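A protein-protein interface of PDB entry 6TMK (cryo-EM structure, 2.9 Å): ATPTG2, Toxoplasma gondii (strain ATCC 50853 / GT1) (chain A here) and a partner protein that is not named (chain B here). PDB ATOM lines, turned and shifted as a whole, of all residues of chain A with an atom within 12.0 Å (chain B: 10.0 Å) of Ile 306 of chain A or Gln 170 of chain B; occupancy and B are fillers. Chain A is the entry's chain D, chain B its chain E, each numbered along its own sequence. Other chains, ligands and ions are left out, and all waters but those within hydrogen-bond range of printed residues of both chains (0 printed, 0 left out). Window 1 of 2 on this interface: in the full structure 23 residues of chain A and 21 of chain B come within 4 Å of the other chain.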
ATOM      1  N   ARG A 298     -32.725 -22.649  -6.225  1.00  0.00           N
ATOM      2  CA  ARG A 298     -31.350 -23.095  -6.414  1.00  0.00           C
ATOM      3  C   ARG A 298     -30.915 -24.072  -5.334  1.00  0.00           C
ATOM      4  O   ARG A 298     -30.089 -24.953  -5.586  1.00  0.00           O
ATOM      5  CB  ARG A 298     -30.434 -21.877  -6.420  1.00  0.00           C
ATOM      6  CG  ARG A 298     -29.029 -22.100  -6.908  1.00  0.00           C
ATOM      7  CD  ARG A 298     -28.181 -20.928  -6.510  1.00  0.00           C
ATOM      8  NE  ARG A 298     -28.766 -19.690  -7.001  1.00  0.00           N
ATOM      9  CZ  ARG A 298     -28.728 -19.302  -8.270  1.00  0.00           C
ATOM     10  NH1 ARG A 298     -28.119 -20.046  -9.177  1.00  0.00           N
ATOM     11  NH2 ARG A 298     -29.302 -18.167  -8.630  1.00  0.00           N
ATOM     12  N   MET A 299     -31.462 -23.929  -4.130  1.00  0.00           N
ATOM     13  CA  MET A 299     -31.114 -24.809  -3.023  1.00  0.00           C
ATOM     14  C   MET A 299     -31.401 -26.269  -3.339  1.00  0.00           C
ATOM     15  O   MET A 299     -30.758 -27.164  -2.781  1.00  0.00           O
ATOM     16  CB  MET A 299     -31.882 -24.378  -1.786  1.00  0.00           C
ATOM     17  CG  MET A 299     -31.378 -24.946  -0.500  1.00  0.00           C
ATOM     18  SD  MET A 299     -32.586 -24.697   0.800  1.00  0.00           S
ATOM     19  CE  MET A 299     -31.533 -24.921   2.211  1.00  0.00           C
ATOM     20  N   MET A 300     -32.347 -26.531  -4.234  1.00  0.00           N
ATOM     21  CA  MET A 300     -32.755 -27.889  -4.553  1.00  0.00           C
ATOM     22  C   MET A 300     -31.820 -28.580  -5.529  1.00  0.00           C
ATOM     23  O   MET A 300     -31.911 -29.799  -5.690  1.00  0.00           O
ATOM     24  CB  MET A 300     -34.161 -27.856  -5.131  1.00  0.00           C
ATOM     25  CG  MET A 300     -35.216 -27.553  -4.102  1.00  0.00           C
ATOM     26  SD  MET A 300     -36.788 -27.099  -4.842  1.00  0.00           S
ATOM     27  CE  MET A 300     -37.125 -28.600  -5.723  1.00  0.00           C
ATOM     28  N   PHE A 301     -30.946 -27.833  -6.192  1.00  0.00           N
ATOM     29  CA  PHE A 301     -29.971 -28.374  -7.122  1.00  0.00           C
ATOM     30  C   PHE A 301     -28.573 -28.427  -6.516  1.00  0.00           C
ATOM     31  O   PHE A 301     -27.582 -28.261  -7.230  1.00  0.00           O
ATOM     32  CB  PHE A 301     -29.994 -27.543  -8.400  1.00  0.00           C
ATOM     33  CG  PHE A 301     -31.370 -27.365  -8.958  1.00  0.00           C
ATOM     34  CD1 PHE A 301     -31.949 -28.356  -9.716  1.00  0.00           C
ATOM     35  CD2 PHE A 301     -32.099 -26.226  -8.693  1.00  0.00           C
ATOM     36  CE1 PHE A 301     -33.215 -28.206 -10.214  1.00  0.00           C
ATOM     37  CE2 PHE A 301     -33.365 -26.079  -9.189  1.00  0.00           C
ATOM     38  CZ  PHE A 301     -33.922 -27.070  -9.950  1.00  0.00           C
ATOM     39  N   THR A 302     -28.478 -28.681  -5.212  1.00  0.00           N
ATOM     40  CA  THR A 302     -27.215 -28.642  -4.496  1.00  0.00           C
ATOM     41  C   THR A 302     -27.142 -29.773  -3.484  1.00  0.00           C
ATOM     42  O   THR A 302     -28.141 -30.114  -2.850  1.00  0.00           O
ATOM     43  CB  THR A 302     -27.036 -27.315  -3.749  1.00  0.00           C
ATOM     44  OG1 THR A 302     -28.034 -27.194  -2.731  1.00  0.00           O
ATOM     45  CG2 THR A 302     -27.168 -26.158  -4.689  1.00  0.00           C
ATOM     46  N   ASP A 303     -25.952 -30.356  -3.344  1.00  0.00           N
ATOM     47  CA  ASP A 303     -25.718 -31.299  -2.258  1.00  0.00           C
ATOM     48  C   ASP A 303     -25.416 -30.584  -0.944  1.00  0.00           C
ATOM     49  O   ASP A 303     -25.698 -31.126   0.126  1.00  0.00           O
ATOM     50  CB  ASP A 303     -24.574 -32.238  -2.636  1.00  0.00           C
ATOM     51  CG  ASP A 303     -25.059 -33.506  -3.309  1.00  0.00           C
ATOM     52  OD1 ASP A 303     -26.110 -34.037  -2.894  1.00  0.00           O
ATOM     53  OD2 ASP A 303     -24.391 -33.970  -4.255  1.00  0.00           O
ATOM     54  N   VAL A 304     -24.843 -29.384  -1.006  1.00  0.00           N
ATOM     55  CA  VAL A 304     -24.564 -28.571   0.169  1.00  0.00           C
ATOM     56  C   VAL A 304     -24.863 -27.126  -0.192  1.00  0.00           C
ATOM     57  O   VAL A 304     -24.741 -26.718  -1.350  1.00  0.00           O
ATOM     58  CB  VAL A 304     -23.110 -28.714   0.680  1.00  0.00           C
ATOM     59  CG1 VAL A 304     -22.915 -30.010   1.375  1.00  0.00           C
ATOM     60  CG2 VAL A 304     -22.142 -28.635  -0.456  1.00  0.00           C
ATOM     61  N   PHE A 305     -25.234 -26.342   0.815  1.00  0.00           N
ATOM     62  CA  PHE A 305     -25.601 -24.952   0.604  1.00  0.00           C
ATOM     63  C   PHE A 305     -25.182 -24.158   1.829  1.00  0.00           C
ATOM     64  O   PHE A 305     -25.568 -24.502   2.949  1.00  0.00           O
ATOM     65  CB  PHE A 305     -27.105 -24.811   0.354  1.00  0.00           C
ATOM     66  CG  PHE A 305     -27.491 -23.562  -0.366  1.00  0.00           C
ATOM     67  CD1 PHE A 305     -27.901 -22.446   0.327  1.00  0.00           C
ATOM     68  CD2 PHE A 305     -27.486 -23.518  -1.744  1.00  0.00           C
ATOM     69  CE1 PHE A 305     -28.260 -21.313  -0.334  1.00  0.00           C
ATOM     70  CE2 PHE A 305     -27.855 -22.379  -2.410  1.00  0.00           C
ATOM     71  CZ  PHE A 305     -28.248 -21.281  -1.708  1.00  0.00           C
ATOM     72  N   ILE A 306     -24.398 -23.112   1.613  1.00  0.00           N
ATOM     73  CA  ILE A 306     -23.917 -22.233   2.669  1.00  0.00           C
ATOM     74  C   ILE A 306     -24.466 -20.834   2.414  1.00  0.00           C
ATOM     75  O   ILE A 306     -23.938 -20.090   1.589  1.00  0.00           O
ATOM     76  CB  ILE A 306     -22.382 -22.219   2.755  1.00  0.00           C
ATOM     77  CG1 ILE A 306     -21.860 -23.558   3.245  1.00  0.00           C
ATOM     78  CG2 ILE A 306     -21.929 -21.142   3.689  1.00  0.00           C
ATOM     79  CD1 ILE A 306     -20.502 -23.848   2.781  1.00  0.00           C
ATOM     80  N   PRO A 307     -25.536 -20.443   3.098  1.00  0.00           N
ATOM     81  CA  PRO A 307     -26.227 -19.203   2.739  1.00  0.00           C
ATOM     82  C   PRO A 307     -25.426 -17.962   3.094  1.00  0.00           C
ATOM     83  O   PRO A 307     -24.373 -18.004   3.733  1.00  0.00           O
ATOM     84  CB  PRO A 307     -27.503 -19.262   3.579  1.00  0.00           C
ATOM     85  CG  PRO A 307     -27.653 -20.661   3.962  1.00  0.00           C
ATOM     86  CD  PRO A 307     -26.274 -21.159   4.144  1.00  0.00           C
ATOM     87  N   THR A 308     -25.974 -16.833   2.666  1.00  0.00           N
ATOM     88  CA  THR A 308     -25.373 -15.536   2.892  1.00  0.00           C
ATOM     89  C   THR A 308     -25.420 -15.151   4.364  1.00  0.00           C
ATOM     90  O   THR A 308     -26.114 -15.757   5.183  1.00  0.00           O
ATOM     91  CB  THR A 308     -26.102 -14.458   2.101  1.00  0.00           C
ATOM     92  OG1 THR A 308     -27.458 -14.383   2.551  1.00  0.00           O
ATOM     93  CG2 THR A 308     -26.086 -14.769   0.646  1.00  0.00           C
ATOM     94  N   THR A 309     -24.669 -14.109   4.683  1.00  0.00           N
ATOM     95  CA  THR A 309     -24.705 -13.455   5.978  1.00  0.00           C
ATOM     96  C   THR A 309     -25.429 -12.126   5.830  1.00  0.00           C
ATOM     97  O   THR A 309     -25.071 -11.314   4.970  1.00  0.00           O
ATOM     98  CB  THR A 309     -23.291 -13.231   6.514  1.00  0.00           C
ATOM     99  OG1 THR A 309     -22.609 -14.488   6.621  1.00  0.00           O
ATOM    100  CG2 THR A 309     -23.337 -12.563   7.852  1.00  0.00           C
ATOM    101  N   LYS A 310     -26.449 -11.906   6.650  1.00  0.00           N
ATOM    102  CA  LYS A 310     -27.227 -10.671   6.557  1.00  0.00           C
ATOM    103  C   LYS A 310     -27.843 -10.260   7.894  1.00  0.00           C
ATOM    104  O   LYS A 310     -28.649 -10.980   8.480  1.00  0.00           O
ATOM    105  CB  LYS A 310     -28.317 -10.810   5.501  1.00  0.00           C
ATOM    106  CG  LYS A 310     -28.858  -9.482   4.985  1.00  0.00           C
ATOM    107  CD  LYS A 310     -28.010  -8.936   3.843  1.00  0.00           C
ATOM    108  CE  LYS A 310     -28.314  -7.473   3.549  1.00  0.00           C
ATOM    109  NZ  LYS A 310     -27.799  -6.529   4.585  1.00  0.00           N
ATOM    110  OXT LYS A 310     -27.553  -9.185   8.416  1.00  0.00           O
ATOM    111  N   ASP B 166     -13.516  -2.997   3.579  1.00  0.00           N
ATOM    112  CA  ASP B 166     -12.879  -4.132   4.217  1.00  0.00           C
ATOM    113  C   ASP B 166     -13.859  -4.863   5.126  1.00  0.00           C
ATOM    114  O   ASP B 166     -14.855  -4.307   5.595  1.00  0.00           O
ATOM    115  CB  ASP B 166     -11.655  -3.677   5.010  1.00  0.00           C
ATOM    116  CG  ASP B 166     -11.995  -2.675   6.089  1.00  0.00           C
ATOM    117  OD1 ASP B 166     -13.162  -2.239   6.157  1.00  0.00           O
ATOM    118  OD2 ASP B 166     -11.089  -2.313   6.866  1.00  0.00           O
ATOM    119  N   HIS B 167     -13.563  -6.139   5.358  1.00  0.00           N
ATOM    120  CA  HIS B 167     -14.333  -6.990   6.259  1.00  0.00           C
ATOM    121  C   HIS B 167     -15.806  -7.020   5.855  1.00  0.00           C
ATOM    122  O   HIS B 167     -16.705  -6.681   6.625  1.00  0.00           O
ATOM    123  CB  HIS B 167     -14.154  -6.550   7.712  1.00  0.00           C
ATOM    124  CG  HIS B 167     -12.781  -6.802   8.243  1.00  0.00           C
ATOM    125  ND1 HIS B 167     -12.295  -8.072   8.465  1.00  0.00           N
ATOM    126  CD2 HIS B 167     -11.787  -5.952   8.590  1.00  0.00           C
ATOM    127  CE1 HIS B 167     -11.061  -7.993   8.926  1.00  0.00           C
ATOM    128  NE2 HIS B 167     -10.729  -6.717   9.013  1.00  0.00           N
ATOM    129  N   GLY B 168     -16.034  -7.451   4.631  1.00  0.00           N
ATOM    130  CA  GLY B 168     -17.371  -7.489   4.099  1.00  0.00           C
ATOM    131  C   GLY B 168     -18.089  -8.773   4.433  1.00  0.00           C
ATOM    132  O   GLY B 168     -17.488  -9.772   4.817  1.00  0.00           O
ATOM    133  N   MET B 169     -19.400  -8.731   4.271  1.00  0.00           N
ATOM    134  CA  MET B 169     -20.245  -9.877   4.552  1.00  0.00           C
ATOM    135  C   MET B 169     -20.372 -10.770   3.331  1.00  0.00           C
ATOM    136  O   MET B 169     -20.080 -10.379   2.201  1.00  0.00           O
ATOM    137  CB  MET B 169     -21.639  -9.441   4.995  1.00  0.00           C
ATOM    138  CG  MET B 169     -21.712  -8.838   6.383  1.00  0.00           C
ATOM    139  SD  MET B 169     -23.365  -8.910   7.090  1.00  0.00           S
ATOM    140  CE  MET B 169     -24.293  -7.993   5.867  1.00  0.00           C
ATOM    141  N   GLN B 170     -20.801 -11.997   3.582  1.00  0.00           N
ATOM    142  CA  GLN B 170     -21.037 -12.938   2.507  1.00  0.00           C
ATOM    143  C   GLN B 170     -22.258 -12.472   1.726  1.00  0.00           C
ATOM    144  O   GLN B 170     -23.369 -12.411   2.261  1.00  0.00           O
ATOM    145  CB  GLN B 170     -21.233 -14.334   3.067  1.00  0.00           C
ATOM    146  CG  GLN B 170     -20.842 -15.431   2.124  1.00  0.00           C
ATOM    147  CD  GLN B 170     -21.350 -16.775   2.572  1.00  0.00           C
ATOM    148  OE1 GLN B 170     -21.185 -17.162   3.724  1.00  0.00           O
ATOM    149  NE2 GLN B 170     -22.004 -17.481   1.671  1.00  0.00           N
ATOM    150  N   TYR B 171     -22.041 -12.145   0.462  1.00  0.00           N
ATOM    151  CA  TYR B 171     -23.031 -11.526  -0.403  1.00  0.00           C
ATOM    152  C   TYR B 171     -23.719 -12.526  -1.310  1.00  0.00           C
ATOM    153  O   TYR B 171     -24.896 -12.352  -1.631  1.00  0.00           O
ATOM    154  CB  TYR B 171     -22.352 -10.431  -1.228  1.00  0.00           C
ATOM    155  CG  TYR B 171     -23.236  -9.317  -1.701  1.00  0.00           C
ATOM    156  CD1 TYR B 171     -23.602  -9.214  -3.031  1.00  0.00           C
ATOM    157  CD2 TYR B 171     -23.685  -8.353  -0.819  1.00  0.00           C
ATOM    158  CE1 TYR B 171     -24.398  -8.188  -3.472  1.00  0.00           C
ATOM    159  CE2 TYR B 171     -24.486  -7.315  -1.251  1.00  0.00           C
ATOM    160  CZ  TYR B 171     -24.842  -7.242  -2.578  1.00  0.00           C
ATOM    161  OH  TYR B 171     -25.638  -6.209  -3.012  1.00  0.00           O
ATOM    162  N   SER B 172     -23.003 -13.558  -1.731  1.00  0.00           N
ATOM    163  CA  SER B 172     -23.524 -14.624  -2.564  1.00  0.00           C
ATOM    164  C   SER B 172     -23.396 -15.935  -1.802  1.00  0.00           C
ATOM    165  O   SER B 172     -22.584 -16.069  -0.885  1.00  0.00           O
ATOM    166  CB  SER B 172     -22.784 -14.702  -3.906  1.00  0.00           C
ATOM    167  OG  SER B 172     -23.047 -13.569  -4.706  1.00  0.00           O
ATOM    168  N   SER B 173     -24.210 -16.903  -2.193  1.00  0.00           N
ATOM    169  CA  SER B 173     -24.212 -18.194  -1.533  1.00  0.00           C
ATOM    170  C   SER B 173     -23.104 -19.089  -2.077  1.00  0.00           C
ATOM    171  O   SER B 173     -22.635 -18.937  -3.207  1.00  0.00           O
ATOM    172  CB  SER B 173     -25.573 -18.865  -1.690  1.00  0.00           C
ATOM    173  OG  SER B 173     -26.622 -17.966  -1.405  1.00  0.00           O
ATOM    174  N   ILE B 174     -22.695 -20.043  -1.248  1.00  0.00           N
ATOM    175  CA  ILE B 174     -21.696 -21.038  -1.602  1.00  0.00           C
ATOM    176  C   ILE B 174     -22.380 -22.393  -1.601  1.00  0.00           C
ATOM    177  O   ILE B 174     -23.109 -22.725  -0.661  1.00  0.00           O
ATOM    178  CB  ILE B 174     -20.514 -21.030  -0.618  1.00  0.00           C
ATOM    179  CG1 ILE B 174     -19.700 -19.752  -0.757  1.00  0.00           C
ATOM    180  CG2 ILE B 174     -19.600 -22.204  -0.872  1.00  0.00           C
ATOM    181  CD1 ILE B 174     -19.050 -19.335   0.511  1.00  0.00           C
ATOM    182  N   TYR B 175     -22.144 -23.173  -2.646  1.00  0.00           N
ATOM    183  CA  TYR B 175     -22.845 -24.435  -2.802  1.00  0.00           C
ATOM    184  C   TYR B 175     -22.081 -25.339  -3.752  1.00  0.00           C
ATOM    185  O   TYR B 175     -21.179 -24.912  -4.474  1.00  0.00           O
ATOM    186  CB  TYR B 175     -24.280 -24.216  -3.291  1.00  0.00           C
ATOM    187  CG  TYR B 175     -24.400 -23.465  -4.589  1.00  0.00           C
ATOM    188  CD1 TYR B 175     -24.343 -24.121  -5.799  1.00  0.00           C
ATOM    189  CD2 TYR B 175     -24.581 -22.098  -4.601  1.00  0.00           C
ATOM    190  CE1 TYR B 175     -24.453 -23.442  -6.973  1.00  0.00           C
ATOM    191  CE2 TYR B 175     -24.693 -21.414  -5.771  1.00  0.00           C
ATOM    192  CZ  TYR B 175     -24.629 -22.088  -6.958  1.00  0.00           C
ATOM    193  OH  TYR B 175     -24.743 -21.395  -8.133  1.00  0.00           O
ATOM    194  N   TRP B 176     -22.464 -26.609  -3.725  1.00  0.00           N
ATOM    195  CA  TRP B 176     -21.932 -27.629  -4.613  1.00  0.00           C
ATOM    196  C   TRP B 176     -23.106 -28.308  -5.290  1.00  0.00           C
ATOM    197  O   TRP B 176     -23.992 -28.840  -4.616  1.00  0.00           O
ATOM    198  CB  TRP B 176     -21.097 -28.651  -3.847  1.00  0.00           C
ATOM    199  CG  TRP B 176     -20.184 -29.452  -4.703  1.00  0.00           C
ATOM    200  CD1 TRP B 176     -20.381 -30.719  -5.145  1.00  0.00           C
ATOM    201  CD2 TRP B 176     -18.925 -29.039  -5.223  1.00  0.00           C
ATOM    202  NE1 TRP B 176     -19.324 -31.123  -5.906  1.00  0.00           N
ATOM    203  CE2 TRP B 176     -18.413 -30.106  -5.973  1.00  0.00           C
ATOM    204  CE3 TRP B 176     -18.180 -27.867  -5.131  1.00  0.00           C
ATOM    205  CZ2 TRP B 176     -17.195 -30.040  -6.618  1.00  0.00           C
ATOM    206  CZ3 TRP B 176     -16.979 -27.803  -5.770  1.00  0.00           C
ATOM    207  CH2 TRP B 176     -16.493 -28.879  -6.506  1.00  0.00           C
ATOM    208  N   GLU B 177     -23.120 -28.272  -6.613  1.00  0.00           N
ATOM    209  CA  GLU B 177     -24.200 -28.896  -7.353  1.00  0.00           C
ATOM    210  C   GLU B 177     -24.108 -30.409  -7.261  1.00  0.00           C
ATOM    211  O   GLU B 177     -23.039 -30.983  -7.052  1.00  0.00           O
ATOM    212  CB  GLU B 177     -24.181 -28.449  -8.811  1.00  0.00           C
ATOM    213  CG  GLU B 177     -24.617 -27.019  -9.003  1.00  0.00           C
ATOM    214  CD  GLU B 177     -24.722 -26.615 -10.456  1.00  0.00           C
ATOM    215  OE1 GLU B 177     -25.029 -27.479 -11.302  1.00  0.00           O
ATOM    216  OE2 GLU B 177     -24.511 -25.421 -10.752  1.00  0.00           O
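Printed residues of chain B within 4 Å of Ile 306 of chain A: Gln 170 (3.2 Å), Ser 173 (3.7 Å) and Ile 174 (2.6 Å).
Of chain A, only Ile 306 (3.2 Å), Pro 307 (3.2 Å), Thr 308 (3.4 Å) and Thr 309 (3.2 Å) come within 4 Å of Gln 170 of chain B.
Of the printed residues of chain B, Pro 307 of chain A touches Gln 170.
Thr 308 of chain A touches just these residues of chain B: Gln 170, Tyr 171, Ser 172 and Ser 173.
Thr 309 of chain A touches two residues of chain B.
Printed residues of chain A within 4 Å of Ser 172 of chain B: Thr 308 (3.8 Å).
Printed residues of chain B within 4 Å of Thr 302 of chain A: Tyr 175 and Trp 176.
Printed residues of chain A within 4 Å of Tyr 171 of chain B: Thr 308 (3.5 Å).
His 167 of chain B touches none of the printed residues of chain A.
Met 300 of chain A touches none of the printed residues of chain B.
The nearest printed residue of chain A that does not touch Met 169 of chain B is Lys 310 of chain A (4.01 Å).
O of Ile 306 of chain A lies within hydrogen-bond range of NE2 of Gln 170 of chain B, 3.2 Å away.
The side-chain amide nitrogen (NE2) of Gln 170 of chain B sits at hydrogen-bond distance from the backbone carbonyl oxygen (O) of Pro 307 of chain A, at 3.2 Å.
O of Gln 170 of chain B lies within hydrogen-bond range of N of Thr 309 of chain A, at 3.2 Å.
O of Ile 174 of chain B is in hydrogen-bond range of N of Ile 306 of chain A.
N of Asp 303 of chain A lies within hydrogen-bond range of O of Trp 176 of chain B (2.8 Å).
The backbone NH of Trp 176 of chain B sits at hydrogen-bond distance from the backbone carbonyl oxygen of Val 304 of chain A.
The side-chain sulfur (SD) of Met 169 of chain B lies close to the backbone carbonyl oxygen (O) of Thr 309 of chain A, 3.6 Å away.
Among the printed residues, pairs that only touch across the chains: Arg 298 of chain A with Tyr 175 of chain B, Phe 301 of chain A with Glu 177 of chain B, Thr 302 of chain A with Tyr 175 of chain B, Thr 302 of chain A with Trp 176 of chain B, Val 304 of chain A with Tyr 175 of chain B, Phe 305 of chain A with Ser 173 of chain B, Phe 305 of chain A with Ile 174 of chain B, Phe 305 of chain A with Tyr 175 of chain B, Ile 306 of chain A with Ser 173 of chain B, Thr 308 of chain A with Gln 170 of chain B, Thr 308 of chain A with Tyr 171 of chain B, Thr 308 of chain A with Ser 172 of chain B and Thr 308 of chain A with Ser 173 of chain B.
Of the 12 printed residues of chain B, 9 touch a printed residue of chain A.
Hydrophobic or aromatic side chains of chain B within 4 Å of the printed part of chain A: Met 169, Tyr 175 and Trp 176.
Of the 13 printed residues of chain A, 10 touch a printed residue of chain B.
The backbone carbonyl oxygen (O) of Ser 172 of chain B lies within hydrogen-bond range of the side-chain amide nitrogen (NE2) of Gln 170 of chain B, at 3.0 Å.
The backbone carbonyl oxygen (O) of Met 299 of chain A is in hydrogen-bond range of the side-chain hydroxyl (OG1) of Thr 302 of chain A.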
